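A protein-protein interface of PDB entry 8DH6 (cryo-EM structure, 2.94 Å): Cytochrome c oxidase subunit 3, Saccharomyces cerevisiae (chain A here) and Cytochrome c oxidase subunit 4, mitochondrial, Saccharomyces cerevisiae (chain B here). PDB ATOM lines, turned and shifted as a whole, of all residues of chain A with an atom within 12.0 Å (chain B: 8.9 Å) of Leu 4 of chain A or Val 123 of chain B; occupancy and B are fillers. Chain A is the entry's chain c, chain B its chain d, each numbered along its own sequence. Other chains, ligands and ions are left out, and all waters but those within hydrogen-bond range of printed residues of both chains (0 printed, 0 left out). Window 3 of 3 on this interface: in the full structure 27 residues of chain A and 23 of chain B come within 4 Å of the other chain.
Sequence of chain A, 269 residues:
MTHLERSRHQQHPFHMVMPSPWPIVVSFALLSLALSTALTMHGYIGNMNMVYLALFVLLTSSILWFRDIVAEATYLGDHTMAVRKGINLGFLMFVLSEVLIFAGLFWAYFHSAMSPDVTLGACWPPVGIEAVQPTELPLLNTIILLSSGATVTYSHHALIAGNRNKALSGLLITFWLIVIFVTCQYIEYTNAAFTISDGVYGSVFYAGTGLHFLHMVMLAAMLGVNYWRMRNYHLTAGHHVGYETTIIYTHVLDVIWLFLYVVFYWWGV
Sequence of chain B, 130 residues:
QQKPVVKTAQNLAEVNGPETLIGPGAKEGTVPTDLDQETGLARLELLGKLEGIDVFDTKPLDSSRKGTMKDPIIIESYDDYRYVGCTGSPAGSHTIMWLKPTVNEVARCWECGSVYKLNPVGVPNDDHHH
The side-chain hydroxyl (OG) of Ser 7 of chain A is in hydrogen-bond range of the backbone carbonyl oxygen (O) of Val 123 of chain B.
A ring nitrogen (ND1) of His 3 of chain A sits at hydrogen-bond distance from the side-chain hydroxyl of Tyr 78 of chain B, 3.3 Å away.
OE2 of Glu 5 of chain A sits at hydrogen-bond distance from N of Gly 17 of chain B, 3.1 Å away.
The side-chain hydroxyl (OG) of Ser 7 of chain A is in hydrogen-bond range of the backbone carbonyl oxygen (O) of Gly 122 of chain B.
Printed residues of chain B that touch a printed residue of chain A: Val 15, Asn 16, Gly 17, Tyr 78, Val 121, Gly 122 and Val 123.
Hydrophobic or aromatic side chains of chain B that line the printed part of chain A: Tyr 78, Val 121 and Val 123.
Of the 11 printed residues of chain A, 7 touch a printed residue of chain B.
Hydrophobic or aromatic side chains of chain A that line the printed part of chain B: His 3 and Leu 4.
Among the printed residues, no Asp or Glu carboxylate lies within 4 Å of a Lys or Arg side-chain nitrogen of the other chain.
Of the printed residues of chain B, His 3 of chain A touches Tyr 78 (3.3 Å) and Val 121 (3.4 Å).
Leu 4 of chain A touches one residue of chain B.
Of the printed residues of chain B, Ser 7 of chain A touches Tyr 78, Gly 122 and Val 123.
Printed residues of chain A within 4 Å of Gly 17 of chain B: Glu 5 (3.1 Å) and Arg 8 (3.3 Å).
Val 121 of chain B touches one residue of chain A.
Gly 122 of chain B touches just one residue of chain A: Ser 7 (3.0 Å).
Pro 124 of chain B touches none of the printed residues of chain A.
The nearest printed residue of chain A that does not touch Asn 16 of chain B is His 9 of chain A (6.2 Å).
The side-chain carboxylate (OE2) of Glu 5 of chain A lies within salt-bridge range of the guanidinium group (NE) of Arg 8 of chain A (3.3 Å).
SD of Met 1 of chain A is in hydrogen-bond range of N of Arg 6 of chain A, 3.4 Å away.
The side-chain amide nitrogen (NE2) of Gln 11 of chain A sits at hydrogen-bond distance from the backbone carbonyl oxygen (O) of Arg 6 of chain A, 3.0 Å away.
The backbone carbonyl oxygen (O) of Glu 5 of chain A lies within hydrogen-bond range of a ring nitrogen (ND1) of His 9 of chain A (3.1 Å).
N of Val 121 of chain B is in hydrogen-bond range of O of Ser 77 of chain B, at 2.5 Å.
Among the printed residues, pairs that only touch across the chains: His 3 of chain A with Val 121 of chain B (3.4 Å), Leu 4 of chain A with Val 123 of chain B (3.5 Å), Glu 5 of chain A with Val 15 of chain B (3.1 Å), Glu 5 of chain A with Asn 16 of chain B (3.4 Å), Arg 6 of chain A with Tyr 78 of chain B (3.2 Å), Ser 7 of chain A with Tyr 78 of chain B (3.9 Å), Arg 8 of chain A with Asn 16 of chain B (3.9 Å), Arg 8 of chain A with Gly 17 of chain B (3.3 Å) and Gln 11 of chain A with Tyr 78 of chain B (3.2 Å).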
ATOM      1  N   MET A   1       0.544  27.784 -31.784  1.00  0.00           N
ATOM      2  CA  MET A   1       0.573  27.191 -30.455  1.00  0.00           C
ATOM      3  C   MET A   1       1.764  27.706 -29.661  1.00  0.00           C
ATOM      4  O   MET A   1       2.610  28.421 -30.191  1.00  0.00           O
ATOM      5  CB  MET A   1       0.634  25.668 -30.544  1.00  0.00           C
ATOM      6  CG  MET A   1       1.906  25.144 -31.180  1.00  0.00           C
ATOM      7  SD  MET A   1       1.896  23.354 -31.363  1.00  0.00           S
ATOM      8  CE  MET A   1       0.740  23.172 -32.708  1.00  0.00           C
ATOM      9  N   THR A   2       1.829  27.331 -28.388  1.00  0.00           N
ATOM     10  CA  THR A   2       2.944  27.717 -27.535  1.00  0.00           C
ATOM     11  C   THR A   2       4.162  26.861 -27.874  1.00  0.00           C
ATOM     12  O   THR A   2       4.082  25.890 -28.632  1.00  0.00           O
ATOM     13  CB  THR A   2       2.557  27.594 -26.064  1.00  0.00           C
ATOM     14  OG1 THR A   2       3.612  28.114 -25.246  1.00  0.00           O
ATOM     15  CG2 THR A   2       2.314  26.141 -25.694  1.00  0.00           C
ATOM     16  N   HIS A   3       5.314  27.219 -27.313  1.00  0.00           N
ATOM     17  CA  HIS A   3       6.536  26.450 -27.510  1.00  0.00           C
ATOM     18  C   HIS A   3       6.463  25.100 -26.811  1.00  0.00           C
ATOM     19  O   HIS A   3       6.992  24.104 -27.319  1.00  0.00           O
ATOM     20  CB  HIS A   3       7.739  27.244 -27.000  1.00  0.00           C
ATOM     21  CG  HIS A   3       8.264  28.243 -27.983  1.00  0.00           C
ATOM     22  ND1 HIS A   3       8.170  28.067 -29.346  1.00  0.00           N
ATOM     23  CD2 HIS A   3       8.882  29.434 -27.801  1.00  0.00           C
ATOM     24  CE1 HIS A   3       8.710  29.105 -29.961  1.00  0.00           C
ATOM     25  NE2 HIS A   3       9.151  29.948 -29.045  1.00  0.00           N
ATOM     26  N   LEU A   4       5.796  25.061 -25.653  1.00  0.00           N
ATOM     27  CA  LEU A   4       5.593  23.825 -24.908  1.00  0.00           C
ATOM     28  C   LEU A   4       4.959  22.731 -25.754  1.00  0.00           C
ATOM     29  O   LEU A   4       5.364  21.570 -25.648  1.00  0.00           O
ATOM     30  CB  LEU A   4       4.711  24.099 -23.690  1.00  0.00           C
ATOM     31  CG  LEU A   4       4.662  23.069 -22.563  1.00  0.00           C
ATOM     32  CD1 LEU A   4       6.054  22.685 -22.142  1.00  0.00           C
ATOM     33  CD2 LEU A   4       3.874  23.610 -21.384  1.00  0.00           C
ATOM     34  N   GLU A   5       3.983  23.077 -26.591  1.00  0.00           N
ATOM     35  CA  GLU A   5       3.313  22.091 -27.427  1.00  0.00           C
ATOM     36  C   GLU A   5       4.049  21.828 -28.729  1.00  0.00           C
ATOM     37  O   GLU A   5       4.091  20.681 -29.187  1.00  0.00           O
ATOM     38  CB  GLU A   5       1.888  22.544 -27.737  1.00  0.00           C
ATOM     39  CG  GLU A   5       1.008  21.435 -28.258  1.00  0.00           C
ATOM     40  CD  GLU A   5       1.154  20.157 -27.457  1.00  0.00           C
ATOM     41  OE1 GLU A   5       0.922  20.195 -26.230  1.00  0.00           O
ATOM     42  OE2 GLU A   5       1.501  19.116 -28.052  1.00  0.00           O
ATOM     43  N   ARG A   6       4.625  22.864 -29.343  1.00  0.00           N
ATOM     44  CA  ARG A   6       5.363  22.666 -30.582  1.00  0.00           C
ATOM     45  C   ARG A   6       6.635  21.857 -30.365  1.00  0.00           C
ATOM     46  O   ARG A   6       7.164  21.284 -31.322  1.00  0.00           O
ATOM     47  CB  ARG A   6       5.692  24.017 -31.217  1.00  0.00           C
ATOM     48  CG  ARG A   6       6.163  23.920 -32.653  1.00  0.00           C
ATOM     49  CD  ARG A   6       5.296  22.955 -33.434  1.00  0.00           C
ATOM     50  NE  ARG A   6       5.803  22.719 -34.778  1.00  0.00           N
ATOM     51  CZ  ARG A   6       6.379  21.592 -35.169  1.00  0.00           C
ATOM     52  NH1 ARG A   6       6.542  20.577 -34.339  1.00  0.00           N
ATOM     53  NH2 ARG A   6       6.802  21.480 -36.424  1.00  0.00           N
ATOM     54  N   SER A   7       7.126  21.785 -29.130  1.00  0.00           N
ATOM     55  CA  SER A   7       8.286  20.961 -28.820  1.00  0.00           C
ATOM     56  C   SER A   7       7.980  19.469 -28.821  1.00  0.00           C
ATOM     57  O   SER A   7       8.909  18.666 -28.686  1.00  0.00           O
ATOM     58  CB  SER A   7       8.863  21.361 -27.462  1.00  0.00           C
ATOM     59  OG  SER A   7       9.919  20.496 -27.088  1.00  0.00           O
ATOM     60  N   ARG A   8       6.716  19.079 -28.962  1.00  0.00           N
ATOM     61  CA  ARG A   8       6.305  17.688 -28.833  1.00  0.00           C
ATOM     62  C   ARG A   8       5.976  17.027 -30.167  1.00  0.00           C
ATOM     63  O   ARG A   8       5.215  16.055 -30.185  1.00  0.00           O
ATOM     64  CB  ARG A   8       5.092  17.589 -27.907  1.00  0.00           C
ATOM     65  CG  ARG A   8       5.386  17.929 -26.463  1.00  0.00           C
ATOM     66  CD  ARG A   8       4.158  18.494 -25.778  1.00  0.00           C
ATOM     67  NE  ARG A   8       3.087  17.512 -25.659  1.00  0.00           N
ATOM     68  CZ  ARG A   8       2.559  17.123 -24.509  1.00  0.00           C
ATOM     69  NH1 ARG A   8       2.978  17.617 -23.356  1.00  0.00           N
ATOM     70  NH2 ARG A   8       1.586  16.218 -24.512  1.00  0.00           N
ATOM     71  N   HIS A   9       6.515  17.522 -31.278  1.00  0.00           N
ATOM     72  CA  HIS A   9       6.160  16.994 -32.590  1.00  0.00           C
ATOM     73  C   HIS A   9       7.426  16.872 -33.436  1.00  0.00           C
ATOM     74  O   HIS A   9       8.548  17.002 -32.938  1.00  0.00           O
ATOM     75  CB  HIS A   9       5.076  17.866 -33.238  1.00  0.00           C
ATOM     76  CG  HIS A   9       3.766  17.832 -32.513  1.00  0.00           C
ATOM     77  ND1 HIS A   9       3.528  18.565 -31.370  1.00  0.00           N
ATOM     78  CD2 HIS A   9       2.627  17.143 -32.760  1.00  0.00           C
ATOM     79  CE1 HIS A   9       2.297  18.335 -30.950  1.00  0.00           C
ATOM     80  NE2 HIS A   9       1.729  17.475 -31.775  1.00  0.00           N
ATOM     81  N   GLN A  10       7.237  16.619 -34.733  1.00  0.00           N
ATOM     82  CA  GLN A  10       8.302  16.147 -35.613  1.00  0.00           C
ATOM     83  C   GLN A  10       9.307  17.220 -36.013  1.00  0.00           C
ATOM     84  O   GLN A  10      10.491  16.902 -36.177  1.00  0.00           O
ATOM     85  CB  GLN A  10       7.695  15.538 -36.880  1.00  0.00           C
ATOM     86  CG  GLN A  10       8.598  14.561 -37.611  1.00  0.00           C
ATOM     87  CD  GLN A  10       9.078  13.432 -36.725  1.00  0.00           C
ATOM     88  OE1 GLN A  10       8.287  12.798 -36.028  1.00  0.00           O
ATOM     89  NE2 GLN A  10      10.380  13.175 -36.745  1.00  0.00           N
ATOM     90  N   GLN A  11       8.863  18.466 -36.192  1.00  0.00           N
ATOM     91  CA  GLN A  11       9.631  19.618 -36.677  1.00  0.00           C
ATOM     92  C   GLN A  11       9.880  19.588 -38.180  1.00  0.00           C
ATOM     93  O   GLN A  11      10.455  20.544 -38.711  1.00  0.00           O
ATOM     94  CB  GLN A  11      10.984  19.787 -35.972  1.00  0.00           C
ATOM     95  CG  GLN A  11      10.893  19.890 -34.469  1.00  0.00           C
ATOM     96  CD  GLN A  11      10.514  21.277 -34.015  1.00  0.00           C
ATOM     97  OE1 GLN A  11      10.938  22.272 -34.601  1.00  0.00           O
ATOM     98  NE2 GLN A  11       9.704  21.353 -32.970  1.00  0.00           N
ATOM     99  N   VAL B  15      -4.449  22.058 -29.247  1.00  0.00           N
ATOM    100  CA  VAL B  15      -3.675  20.837 -29.418  1.00  0.00           C
ATOM    101  C   VAL B  15      -2.835  20.607 -28.172  1.00  0.00           C
ATOM    102  O   VAL B  15      -2.044  21.468 -27.769  1.00  0.00           O
ATOM    103  CB  VAL B  15      -2.799  20.925 -30.675  1.00  0.00           C
ATOM    104  CG1 VAL B  15      -2.015  19.643 -30.866  1.00  0.00           C
ATOM    105  CG2 VAL B  15      -3.654  21.216 -31.895  1.00  0.00           C
ATOM    106  N   ASN B  16      -3.022  19.450 -27.538  1.00  0.00           N
ATOM    107  CA  ASN B  16      -2.282  19.088 -26.327  1.00  0.00           C
ATOM    108  C   ASN B  16      -1.936  17.608 -26.470  1.00  0.00           C
ATOM    109  O   ASN B  16      -2.708  16.734 -26.066  1.00  0.00           O
ATOM    110  CB  ASN B  16      -3.106  19.382 -25.074  1.00  0.00           C
ATOM    111  CG  ASN B  16      -2.424  18.941 -23.784  1.00  0.00           C
ATOM    112  OD1 ASN B  16      -1.807  17.880 -23.706  1.00  0.00           O
ATOM    113  ND2 ASN B  16      -2.541  19.771 -22.755  1.00  0.00           N
ATOM    114  N   GLY B  17      -0.774  17.332 -27.050  1.00  0.00           N
ATOM    115  CA  GLY B  17      -0.310  15.977 -27.219  1.00  0.00           C
ATOM    116  C   GLY B  17      -0.833  15.342 -28.489  1.00  0.00           C
ATOM    117  O   GLY B  17      -1.762  15.845 -29.127  1.00  0.00           O
ATOM    118  N   SER B  77      15.866  27.694 -32.071  1.00  0.00           N
ATOM    119  CA  SER B  77      16.034  26.265 -32.285  1.00  0.00           C
ATOM    120  C   SER B  77      15.213  25.487 -31.271  1.00  0.00           C
ATOM    121  O   SER B  77      14.854  26.004 -30.212  1.00  0.00           O
ATOM    122  CB  SER B  77      17.499  25.840 -32.184  1.00  0.00           C
ATOM    123  OG  SER B  77      17.603  24.448 -31.957  1.00  0.00           O
ATOM    124  N   TYR B  78      14.895  24.246 -31.620  1.00  0.00           N
ATOM    125  CA  TYR B  78      14.263  23.327 -30.686  1.00  0.00           C
ATOM    126  C   TYR B  78      15.241  22.306 -30.125  1.00  0.00           C
ATOM    127  O   TYR B  78      14.828  21.420 -29.371  1.00  0.00           O
ATOM    128  CB  TYR B  78      13.083  22.620 -31.359  1.00  0.00           C
ATOM    129  CG  TYR B  78      11.870  23.510 -31.512  1.00  0.00           C
ATOM    130  CD1 TYR B  78      11.866  24.560 -32.421  1.00  0.00           C
ATOM    131  CD2 TYR B  78      10.742  23.318 -30.733  1.00  0.00           C
ATOM    132  CE1 TYR B  78      10.767  25.381 -32.558  1.00  0.00           C
ATOM    133  CE2 TYR B  78       9.639  24.133 -30.866  1.00  0.00           C
ATOM    134  CZ  TYR B  78       9.658  25.164 -31.777  1.00  0.00           C
ATOM    135  OH  TYR B  78       8.562  25.982 -31.911  1.00  0.00           O
ATOM    136  N   ASP B  79      16.519  22.413 -30.479  1.00  0.00           N
ATOM    137  CA  ASP B  79      17.589  21.608 -29.915  1.00  0.00           C
ATOM    138  C   ASP B  79      18.740  22.536 -29.546  1.00  0.00           C
ATOM    139  O   ASP B  79      18.758  23.711 -29.919  1.00  0.00           O
ATOM    140  CB  ASP B  79      18.051  20.521 -30.895  1.00  0.00           C
ATOM    141  CG  ASP B  79      18.824  19.410 -30.211  1.00  0.00           C
ATOM    142  OD1 ASP B  79      18.197  18.610 -29.485  1.00  0.00           O
ATOM    143  OD2 ASP B  79      20.056  19.339 -30.394  1.00  0.00           O
ATOM    144  N   ASP B  80      19.715  22.000 -28.810  1.00  0.00           N
ATOM    145  CA  ASP B  80      20.757  22.852 -28.244  1.00  0.00           C
ATOM    146  C   ASP B  80      21.765  23.330 -29.290  1.00  0.00           C
ATOM    147  O   ASP B  80      22.626  24.157 -28.973  1.00  0.00           O
ATOM    148  CB  ASP B  80      21.457  22.128 -27.090  1.00  0.00           C
ATOM    149  CG  ASP B  80      22.168  20.862 -27.526  1.00  0.00           C
ATOM    150  OD1 ASP B  80      22.093  20.504 -28.718  1.00  0.00           O
ATOM    151  OD2 ASP B  80      22.808  20.220 -26.668  1.00  0.00           O
ATOM    152  N   PRO B 120      17.272  28.366 -27.686  1.00  0.00           N
ATOM    153  CA  PRO B 120      16.434  27.168 -27.806  1.00  0.00           C
ATOM    154  C   PRO B 120      15.012  27.358 -27.302  1.00  0.00           C
ATOM    155  O   PRO B 120      14.749  28.092 -26.348  1.00  0.00           O
ATOM    156  CB  PRO B 120      17.165  26.149 -26.919  1.00  0.00           C
ATOM    157  CG  PRO B 120      18.543  26.672 -26.763  1.00  0.00           C
ATOM    158  CD  PRO B 120      18.387  28.158 -26.752  1.00  0.00           C
ATOM    159  N   VAL B 121      14.081  26.682 -27.969  1.00  0.00           N
ATOM    160  CA  VAL B 121      12.776  26.407 -27.375  1.00  0.00           C
ATOM    161  C   VAL B 121      12.903  25.430 -26.217  1.00  0.00           C
ATOM    162  O   VAL B 121      12.345  25.648 -25.137  1.00  0.00           O
ATOM    163  CB  VAL B 121      11.804  25.865 -28.442  1.00  0.00           C
ATOM    164  CG1 VAL B 121      10.593  25.234 -27.771  1.00  0.00           C
ATOM    165  CG2 VAL B 121      11.375  26.962 -29.384  1.00  0.00           C
ATOM    166  N   GLY B 122      13.639  24.347 -26.434  1.00  0.00           N
ATOM    167  CA  GLY B 122      13.942  23.420 -25.355  1.00  0.00           C
ATOM    168  C   GLY B 122      12.723  22.655 -24.901  1.00  0.00           C
ATOM    169  O   GLY B 122      11.910  22.215 -25.717  1.00  0.00           O
ATOM    170  N   VAL B 123      12.597  22.510 -23.581  1.00  0.00           N
ATOM    171  CA  VAL B 123      11.618  21.672 -22.881  1.00  0.00           C
ATOM    172  C   VAL B 123      11.398  20.372 -23.653  1.00  0.00           C
ATOM    173  O   VAL B 123      10.337  20.166 -24.261  1.00  0.00           O
ATOM    174  CB  VAL B 123      10.307  22.433 -22.584  1.00  0.00           C
ATOM    175  CG1 VAL B 123       9.625  23.005 -23.838  1.00  0.00           C
ATOM    176  CG2 VAL B 123       9.356  21.566 -21.742  1.00  0.00           C
ATOM    177  N   PRO B 124      12.386  19.467 -23.672  1.00  0.00           N
ATOM    178  CA  PRO B 124      12.276  18.207 -24.413  1.00  0.00           C
ATOM    179  C   PRO B 124      11.361  17.198 -23.722  1.00  0.00           C
ATOM    180  O   PRO B 124      10.261  16.949 -24.217  1.00  0.00           O
ATOM    181  CB  PRO B 124      13.717  17.703 -24.449  1.00  0.00           C
ATOM    182  CG  PRO B 124      14.321  18.236 -23.190  1.00  0.00           C
ATOM    183  CD  PRO B 124      13.641  19.550 -22.903  1.00  0.00           C
